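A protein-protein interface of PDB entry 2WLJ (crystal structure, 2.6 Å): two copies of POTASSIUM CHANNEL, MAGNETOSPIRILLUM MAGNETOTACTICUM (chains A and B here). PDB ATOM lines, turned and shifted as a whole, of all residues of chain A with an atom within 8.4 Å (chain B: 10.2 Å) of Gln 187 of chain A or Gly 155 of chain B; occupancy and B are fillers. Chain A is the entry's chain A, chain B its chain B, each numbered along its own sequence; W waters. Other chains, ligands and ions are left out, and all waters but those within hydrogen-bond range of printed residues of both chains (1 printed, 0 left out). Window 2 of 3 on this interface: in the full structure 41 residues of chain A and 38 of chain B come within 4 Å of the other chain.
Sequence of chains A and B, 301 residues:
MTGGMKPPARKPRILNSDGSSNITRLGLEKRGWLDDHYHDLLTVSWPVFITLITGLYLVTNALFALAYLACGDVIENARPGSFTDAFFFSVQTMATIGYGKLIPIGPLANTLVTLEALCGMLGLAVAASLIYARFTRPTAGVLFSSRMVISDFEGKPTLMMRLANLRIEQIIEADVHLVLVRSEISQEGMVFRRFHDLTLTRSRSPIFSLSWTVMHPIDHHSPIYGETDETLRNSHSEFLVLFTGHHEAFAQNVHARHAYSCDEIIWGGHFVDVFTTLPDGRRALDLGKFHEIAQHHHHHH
The side-chain carboxylate of Glu 188 of chain A lies within hydrogen-bond range of the backbone NH of Gly 155 of chain B, at 2.6 Å. The backbone NH of Glu 154 of chain B sits at hydrogen-bond distance from the side-chain carboxylate of Glu 188 of chain A, 2.8 Å away. OE1 of Glu 154 of chain B is in hydrogen-bond range of N of Gln 187 of chain A (3.4 Å).
The backbone NH of Met 190 of chain A is in hydrogen-bond range of the side-chain hydroxyl of Ser 186 of chain A (3.2 Å). The backbone NH of Glu 184 of chain A sits at hydrogen-bond distance from the backbone carbonyl oxygen of Phe 192 of chain A, 2.8 Å away. OG of Ser 186 of chain A sits at hydrogen-bond distance from OE1 of Glu 188 of chain A (3.3 Å).
OE1 of Glu 154 of chain B touches CA of Ser 186 of chain A, 3.8 Å away. Gln 187 of chain A touches Gly 155 of chain B (OE1 to CA, 3.5 Å). Glu 188 of chain A touches Asp 152 of chain B. OE1 of Glu 188 of chain A touches CA of Phe 153 of chain B, at 3.4 Å. Phe 153 of chain B touches Met 190 of chain A (CE1 to CE, 3.6 Å). Phe 192 of chain A touches Phe 153 of chain B (CZ to CZ, 3.6 Å).
Glu 188 of chain A touches four residues of chain B. Of the printed residues of chain B, Met 190 of chain A touches Phe 153 (3.6 Å). Of the printed residues of chain B, Phe 192 of chain A touches Phe 153. Of the printed residues of chain A, Asp 152 of chain B touches Glu 188 (3.8 Å). Printed residues of chain A within 4 Å of Phe 153 of chain B: Glu 188, Met 190 and Phe 192. Of the printed residues of chain A, Glu 154 of chain B touches Ser 186 (3.8 Å), Gln 187 (3.4 Å) and Glu 188 (2.8 Å). Of chain A, only Gln 187 (3.5 Å) and Glu 188 (2.6 Å) come within 4 Å of Gly 155 of chain B. Pro 157 of chain B touches none of the printed residues of chain A. The nearest printed residue of chain A that does not touch Glu 154 of chain B is Phe 192 of chain A (4.4 Å).
Hydrophobic or aromatic side chains of chain A within 4 Å of the printed part of chain B: Met 190 and Phe 192. Printed residues of chain B that touch a printed residue of chain A: Asp 152, Phe 153, Glu 154 and Gly 155. Among the printed residues, 9 pairs touch across the chains.
No position is printed for both chains. Of the 9 pairs that touch across the chains among the printed residues, none has its exchanged pair printed and touching as well.
Water W1 bridges OE1 of Glu 154 of chain B and N of Gln 187 of chain A.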
ATOM      1  N   GLU A 184     -12.308  15.272  13.489  1.00  0.00           N
ATOM      2  CA  GLU A 184     -13.667  14.805  13.469  1.00  0.00           C
ATOM      3  C   GLU A 184     -13.924  13.809  14.592  1.00  0.00           C
ATOM      4  O   GLU A 184     -12.992  13.284  15.215  1.00  0.00           O
ATOM      5  CB  GLU A 184     -13.962  14.236  12.091  1.00  0.00           C
ATOM      6  CG  GLU A 184     -13.849  15.305  11.001  1.00  0.00           C
ATOM      7  CD  GLU A 184     -14.257  14.809   9.610  1.00  0.00           C
ATOM      8  OE1 GLU A 184     -14.706  13.626   9.524  1.00  0.00           O
ATOM      9  OE2 GLU A 184     -14.120  15.603   8.613  1.00  0.00           O
ATOM     10  N   ILE A 185     -15.201  13.595  14.887  1.00  0.00           N
ATOM     11  CA  ILE A 185     -15.608  12.667  15.926  1.00  0.00           C
ATOM     12  C   ILE A 185     -16.350  11.499  15.278  1.00  0.00           C
ATOM     13  O   ILE A 185     -17.350  11.703  14.586  1.00  0.00           O
ATOM     14  CB  ILE A 185     -16.538  13.375  16.923  1.00  0.00           C
ATOM     15  CG1 ILE A 185     -15.837  14.613  17.491  1.00  0.00           C
ATOM     16  CG2 ILE A 185     -16.972  12.431  18.036  1.00  0.00           C
ATOM     17  CD1 ILE A 185     -16.756  15.547  18.291  1.00  0.00           C
ATOM     18  N   SER A 186     -15.875  10.283  15.480  1.00  0.00           N
ATOM     19  CA  SER A 186     -16.585   9.149  14.921  1.00  0.00           C
ATOM     20  C   SER A 186     -17.836   8.778  15.735  1.00  0.00           C
ATOM     21  O   SER A 186     -17.998   9.208  16.887  1.00  0.00           O
ATOM     22  CB  SER A 186     -15.653   7.938  14.823  1.00  0.00           C
ATOM     23  OG  SER A 186     -15.374   7.372  16.091  1.00  0.00           O
ATOM     24  N   GLN A 187     -18.702   7.959  15.137  1.00  0.00           N
ATOM     25  CA  GLN A 187     -19.853   7.397  15.844  1.00  0.00           C
ATOM     26  C   GLN A 187     -19.427   6.710  17.143  1.00  0.00           C
ATOM     27  O   GLN A 187     -20.161   6.690  18.125  1.00  0.00           O
ATOM     28  CB  GLN A 187     -20.600   6.371  14.982  1.00  0.00           C
ATOM     29  CG  GLN A 187     -21.146   6.862  13.611  1.00  0.00           C
ATOM     30  CD  GLN A 187     -22.001   5.783  12.934  1.00  0.00           C
ATOM     31  OE1 GLN A 187     -22.363   4.769  13.564  1.00  0.00           O
ATOM     32  NE2 GLN A 187     -22.322   5.988  11.663  1.00  0.00           N
ATOM     33  N   GLU A 188     -18.250   6.120  17.151  1.00  0.00           N
ATOM     34  CA  GLU A 188     -17.791   5.488  18.366  1.00  0.00           C
ATOM     35  C   GLU A 188     -17.208   6.524  19.336  1.00  0.00           C
ATOM     36  O   GLU A 188     -16.647   6.177  20.372  1.00  0.00           O
ATOM     37  CB  GLU A 188     -16.796   4.377  18.042  1.00  0.00           C
ATOM     38  CG  GLU A 188     -17.391   3.293  17.139  1.00  0.00           C
ATOM     39  CD  GLU A 188     -17.606   3.741  15.671  1.00  0.00           C
ATOM     40  OE1 GLU A 188     -16.827   4.565  15.141  1.00  0.00           O
ATOM     41  OE2 GLU A 188     -18.562   3.241  15.037  1.00  0.00           O
ATOM     42  N   GLY A 189     -17.361   7.801  19.012  1.00  0.00           N
ATOM     43  CA  GLY A 189     -16.859   8.853  19.881  1.00  0.00           C
ATOM     44  C   GLY A 189     -15.347   8.980  19.966  1.00  0.00           C
ATOM     45  O   GLY A 189     -14.807   9.425  20.980  1.00  0.00           O
ATOM     46  N   MET A 190     -14.653   8.581  18.913  1.00  0.00           N
ATOM     47  CA  MET A 190     -13.224   8.790  18.850  1.00  0.00           C
ATOM     48  C   MET A 190     -12.933  10.078  18.071  1.00  0.00           C
ATOM     49  O   MET A 190     -13.578  10.368  17.053  1.00  0.00           O
ATOM     50  CB  MET A 190     -12.535   7.586  18.197  1.00  0.00           C
ATOM     51  CG  MET A 190     -11.104   7.877  17.745  1.00  0.00           C
ATOM     52  SD  MET A 190     -10.322   6.640  16.653  1.00  0.00           S
ATOM     53  CE  MET A 190     -10.954   7.042  15.015  1.00  0.00           C
ATOM     54  N   VAL A 191     -11.983  10.865  18.570  1.00  0.00           N
ATOM     55  CA  VAL A 191     -11.561  12.051  17.855  1.00  0.00           C
ATOM     56  C   VAL A 191     -10.316  11.761  17.046  1.00  0.00           C
ATOM     57  O   VAL A 191      -9.390  11.133  17.543  1.00  0.00           O
ATOM     58  CB  VAL A 191     -11.282  13.236  18.785  1.00  0.00           C
ATOM     59  CG1 VAL A 191     -10.497  14.338  18.035  1.00  0.00           C
ATOM     60  CG2 VAL A 191     -12.594  13.796  19.325  1.00  0.00           C
ATOM     61  N   PHE A 192     -10.298  12.218  15.793  1.00  0.00           N
ATOM     62  CA  PHE A 192      -9.189  11.909  14.893  1.00  0.00           C
ATOM     63  C   PHE A 192      -9.117  12.919  13.738  1.00  0.00           C
ATOM     64  O   PHE A 192     -10.127  13.543  13.370  1.00  0.00           O
ATOM     65  CB  PHE A 192      -9.342  10.486  14.350  1.00  0.00           C
ATOM     66  CG  PHE A 192     -10.470  10.339  13.390  1.00  0.00           C
ATOM     67  CD1 PHE A 192     -10.227  10.315  12.006  1.00  0.00           C
ATOM     68  CD2 PHE A 192     -11.785  10.278  13.846  1.00  0.00           C
ATOM     69  CE1 PHE A 192     -11.289  10.193  11.078  1.00  0.00           C
ATOM     70  CE2 PHE A 192     -12.856  10.163  12.942  1.00  0.00           C
ATOM     71  CZ  PHE A 192     -12.611  10.119  11.543  1.00  0.00           C
ATOM     72  N   SER B 151     -12.449  -3.886  14.062  1.00  0.00           N
ATOM     73  CA  SER B 151     -13.275  -3.264  15.055  1.00  0.00           C
ATOM     74  C   SER B 151     -14.097  -2.143  14.423  1.00  0.00           C
ATOM     75  O   SER B 151     -13.836  -1.737  13.284  1.00  0.00           O
ATOM     76  CB  SER B 151     -12.401  -2.783  16.217  1.00  0.00           C
ATOM     77  OG  SER B 151     -11.781  -1.531  15.988  1.00  0.00           O
ATOM     78  N   ASP B 152     -15.095  -1.652  15.140  1.00  0.00           N
ATOM     79  CA  ASP B 152     -16.019  -0.684  14.573  1.00  0.00           C
ATOM     80  C   ASP B 152     -15.412   0.672  14.314  1.00  0.00           C
ATOM     81  O   ASP B 152     -14.790   1.266  15.203  1.00  0.00           O
ATOM     82  CB  ASP B 152     -17.218  -0.493  15.478  1.00  0.00           C
ATOM     83  CG  ASP B 152     -18.179  -1.661  15.417  1.00  0.00           C
ATOM     84  OD1 ASP B 152     -17.804  -2.710  14.828  1.00  0.00           O
ATOM     85  OD2 ASP B 152     -19.305  -1.528  15.960  1.00  0.00           O
ATOM     86  N   PHE B 153     -15.612   1.169  13.094  1.00  0.00           N
ATOM     87  CA  PHE B 153     -15.313   2.566  12.788  1.00  0.00           C
ATOM     88  C   PHE B 153     -16.434   3.163  11.938  1.00  0.00           C
ATOM     89  O   PHE B 153     -16.873   2.556  10.961  1.00  0.00           O
ATOM     90  CB  PHE B 153     -13.979   2.698  12.110  1.00  0.00           C
ATOM     91  CG  PHE B 153     -13.678   4.081  11.642  1.00  0.00           C
ATOM     92  CD1 PHE B 153     -13.240   5.038  12.530  1.00  0.00           C
ATOM     93  CD2 PHE B 153     -13.844   4.425  10.291  1.00  0.00           C
ATOM     94  CE1 PHE B 153     -12.948   6.324  12.103  1.00  0.00           C
ATOM     95  CE2 PHE B 153     -13.568   5.698   9.856  1.00  0.00           C
ATOM     96  CZ  PHE B 153     -13.107   6.656  10.766  1.00  0.00           C
ATOM     97  N   GLU B 154     -16.919   4.341  12.327  1.00  0.00           N
ATOM     98  CA  GLU B 154     -18.097   4.880  11.678  1.00  0.00           C
ATOM     99  C   GLU B 154     -19.171   3.805  11.541  1.00  0.00           C
ATOM    100  O   GLU B 154     -19.774   3.692  10.478  1.00  0.00           O
ATOM    101  CB  GLU B 154     -17.779   5.384  10.272  1.00  0.00           C
ATOM    102  CG  GLU B 154     -16.812   6.508  10.197  1.00  0.00           C
ATOM    103  CD  GLU B 154     -17.272   7.703  10.963  1.00  0.00           C
ATOM    104  OE1 GLU B 154     -18.141   7.576  11.841  1.00  0.00           O
ATOM    105  OE2 GLU B 154     -16.748   8.793  10.715  1.00  0.00           O
ATOM    106  N   GLY B 155     -19.391   2.995  12.574  1.00  0.00           N
ATOM    107  CA  GLY B 155     -20.495   2.040  12.571  1.00  0.00           C
ATOM    108  C   GLY B 155     -20.359   0.738  11.786  1.00  0.00           C
ATOM    109  O   GLY B 155     -21.282  -0.068  11.791  1.00  0.00           O
ATOM    110  N   LYS B 156     -19.238   0.522  11.103  1.00  0.00           N
ATOM    111  CA  LYS B 156     -18.988  -0.747  10.429  1.00  0.00           C
ATOM    112  C   LYS B 156     -17.773  -1.393  11.055  1.00  0.00           C
ATOM    113  O   LYS B 156     -16.833  -0.688  11.396  1.00  0.00           O
ATOM    114  CB  LYS B 156     -18.626  -0.523   8.943  1.00  0.00           C
ATOM    115  CG  LYS B 156     -19.675   0.101   8.073  1.00  0.00           C
ATOM    116  CD  LYS B 156     -19.214  -0.006   6.642  1.00  0.00           C
ATOM    117  CE  LYS B 156     -20.322   0.314   5.677  1.00  0.00           C
ATOM    118  NZ  LYS B 156     -21.239   1.258   6.351  1.00  0.00           N
ATOM    119  N   PRO B 157     -17.773  -2.731  11.173  1.00  0.00           N
ATOM    120  CA  PRO B 157     -16.521  -3.435  11.418  1.00  0.00           C
ATOM    121  C   PRO B 157     -15.521  -3.033  10.338  1.00  0.00           C
ATOM    122  O   PRO B 157     -15.889  -2.946   9.170  1.00  0.00           O
ATOM    123  CB  PRO B 157     -16.888  -4.918  11.216  1.00  0.00           C
ATOM    124  CG  PRO B 157     -18.384  -4.998  11.343  1.00  0.00           C
ATOM    125  CD  PRO B 157     -18.922  -3.643  10.984  1.00  0.00           C
ATOM    126  N   THR B 158     -14.253  -2.815  10.722  1.00  0.00           N
ATOM    127  CA  THR B 158     -13.244  -2.307   9.801  1.00  0.00           C
ATOM    128  C   THR B 158     -11.899  -3.002  10.029  1.00  0.00           C
ATOM    129  O   THR B 158     -11.463  -3.161  11.169  1.00  0.00           O
ATOM    130  CB  THR B 158     -13.118  -0.801  10.004  1.00  0.00           C
ATOM    131  OG1 THR B 158     -14.386  -0.208   9.717  1.00  0.00           O
ATOM    132  CG2 THR B 158     -12.076  -0.219   9.113  1.00  0.00           C
ATOM    133  N   MET B 160      -7.978  -2.941   9.995  1.00  0.00           N
ATOM    134  CA  MET B 160      -7.033  -1.839  10.021  1.00  0.00           C
ATOM    135  C   MET B 160      -5.692  -2.308  10.419  1.00  0.00           C
ATOM    136  O   MET B 160      -5.567  -3.338  11.048  1.00  0.00           O
ATOM    137  CB  MET B 160      -7.416  -0.790  11.045  1.00  0.00           C
ATOM    138  CG  MET B 160      -8.863  -0.521  11.201  1.00  0.00           C
ATOM    139  SD  MET B 160      -9.044   0.677  12.579  1.00  0.00           S
ATOM    140  CE  MET B 160     -10.781   0.446  13.014  1.00  0.00           C
ATOM    141  N   THR B 201     -10.627   3.490   3.117  1.00  0.00           N
ATOM    142  CA  THR B 201     -11.269   4.785   3.230  1.00  0.00           C
ATOM    143  C   THR B 201     -10.348   5.838   2.579  1.00  0.00           C
ATOM    144  O   THR B 201     -10.809   6.788   1.967  1.00  0.00           O
ATOM    145  CB  THR B 201     -11.591   5.160   4.693  1.00  0.00           C
ATOM    146  OG1 THR B 201     -10.374   5.173   5.428  1.00  0.00           O
ATOM    147  CG2 THR B 201     -12.510   4.142   5.352  1.00  0.00           C
ATOM    148  N   MET B 215      -7.396   1.699   6.656  1.00  0.00           N
ATOM    149  CA  MET B 215      -8.652   1.054   7.076  1.00  0.00           C
ATOM    150  C   MET B 215      -9.451   0.542   5.897  1.00  0.00           C
ATOM    151  O   MET B 215      -9.636   1.254   4.876  1.00  0.00           O
ATOM    152  CB  MET B 215      -9.539   2.051   7.846  1.00  0.00           C
ATOM    153  CG  MET B 215      -8.889   2.654   9.090  1.00  0.00           C
ATOM    154  SD  MET B 215     -10.023   3.866   9.823  1.00  0.00           S
ATOM    155  CE  MET B 215     -10.052   5.122   8.528  1.00  0.00           C
ATOM    156  N   HIS B 216      -9.972  -0.665   6.064  1.00  0.00           N
ATOM    157  CA  HIS B 216     -10.820  -1.260   5.076  1.00  0.00           C
ATOM    158  C   HIS B 216     -12.204  -1.529   5.670  1.00  0.00           C
ATOM    159  O   HIS B 216     -12.356  -2.459   6.475  1.00  0.00           O
ATOM    160  CB  HIS B 216     -10.238  -2.600   4.648  1.00  0.00           C
ATOM    161  CG  HIS B 216     -11.190  -3.404   3.812  1.00  0.00           C
ATOM    162  ND1 HIS B 216     -11.655  -4.645   4.189  1.00  0.00           N
ATOM    163  CD2 HIS B 216     -11.809  -3.111   2.642  1.00  0.00           C
ATOM    164  CE1 HIS B 216     -12.488  -5.103   3.268  1.00  0.00           C
ATOM    165  NE2 HIS B 216     -12.610  -4.182   2.326  1.00  0.00           N
ATOM    166  N   PRO B 217     -13.212  -0.726   5.304  1.00  0.00           N
ATOM    167  CA  PRO B 217     -14.538  -0.973   5.878  1.00  0.00           C
ATOM    168  C   PRO B 217     -15.094  -2.275   5.391  1.00  0.00           C
ATOM    169  O   PRO B 217     -15.194  -2.473   4.183  1.00  0.00           O
ATOM    170  CB  PRO B 217     -15.368   0.188   5.327  1.00  0.00           C
ATOM    171  CG  PRO B 217     -14.325   1.291   5.152  1.00  0.00           C
ATOM    172  CD  PRO B 217     -13.031   0.621   5.626  1.00  0.00           C
ATOM    173  N   ILE B 218     -15.448  -3.185   6.293  1.00  0.00           N
ATOM    174  CA  ILE B 218     -15.994  -4.452   5.844  1.00  0.00           C
ATOM    175  C   ILE B 218     -17.486  -4.281   5.567  1.00  0.00           C
ATOM    176  O   ILE B 218     -18.332  -4.584   6.393  1.00  0.00           O
ATOM    177  CB  ILE B 218     -15.754  -5.569   6.843  1.00  0.00           C
ATOM    178  CG1 ILE B 218     -14.257  -5.729   7.084  1.00  0.00           C
ATOM    179  CG2 ILE B 218     -16.395  -6.882   6.363  1.00  0.00           C
ATOM    180  CD1 ILE B 218     -13.895  -6.535   8.331  1.00  0.00           C
ATOM    181  N   ASP B 219     -17.813  -3.793   4.385  1.00  0.00           N
ATOM    182  CA  ASP B 219     -19.194  -3.605   4.036  1.00  0.00           C
ATOM    183  C   ASP B 219     -19.696  -4.772   3.161  1.00  0.00           C
ATOM    184  O   ASP B 219     -18.998  -5.763   2.975  1.00  0.00           O
ATOM    185  CB  ASP B 219     -19.334  -2.241   3.345  1.00  0.00           C
ATOM    186  CG  ASP B 219     -18.635  -2.192   1.998  1.00  0.00           C
ATOM    187  OD1 ASP B 219     -18.191  -3.248   1.497  1.00  0.00           O
ATOM    188  OD2 ASP B 219     -18.535  -1.089   1.433  1.00  0.00           O
ATOM    189  N   TYR B 225     -16.544  -9.813   4.084  1.00  0.00           N
ATOM    190  CA  TYR B 225     -17.842  -9.678   4.677  1.00  0.00           C
ATOM    191  C   TYR B 225     -18.347 -11.060   5.071  1.00  0.00           C
ATOM    192  O   TYR B 225     -18.484 -11.953   4.234  1.00  0.00           O
ATOM    193  CB  TYR B 225     -18.800  -9.051   3.667  1.00  0.00           C
ATOM    194  CG  TYR B 225     -20.160  -8.735   4.236  1.00  0.00           C
ATOM    195  CD1 TYR B 225     -20.337  -7.606   5.011  1.00  0.00           C
ATOM    196  CD2 TYR B 225     -21.264  -9.563   4.002  1.00  0.00           C
ATOM    197  CE1 TYR B 225     -21.541  -7.298   5.566  1.00  0.00           C
ATOM    198  CE2 TYR B 225     -22.509  -9.249   4.541  1.00  0.00           C
ATOM    199  CZ  TYR B 225     -22.627  -8.099   5.334  1.00  0.00           C
ATOM    200  OH  TYR B 225     -23.806  -7.695   5.911  1.00  0.00           O
HETATM  201  O   HOH W   1     -19.956   9.263  12.944  1.00  0.00           O
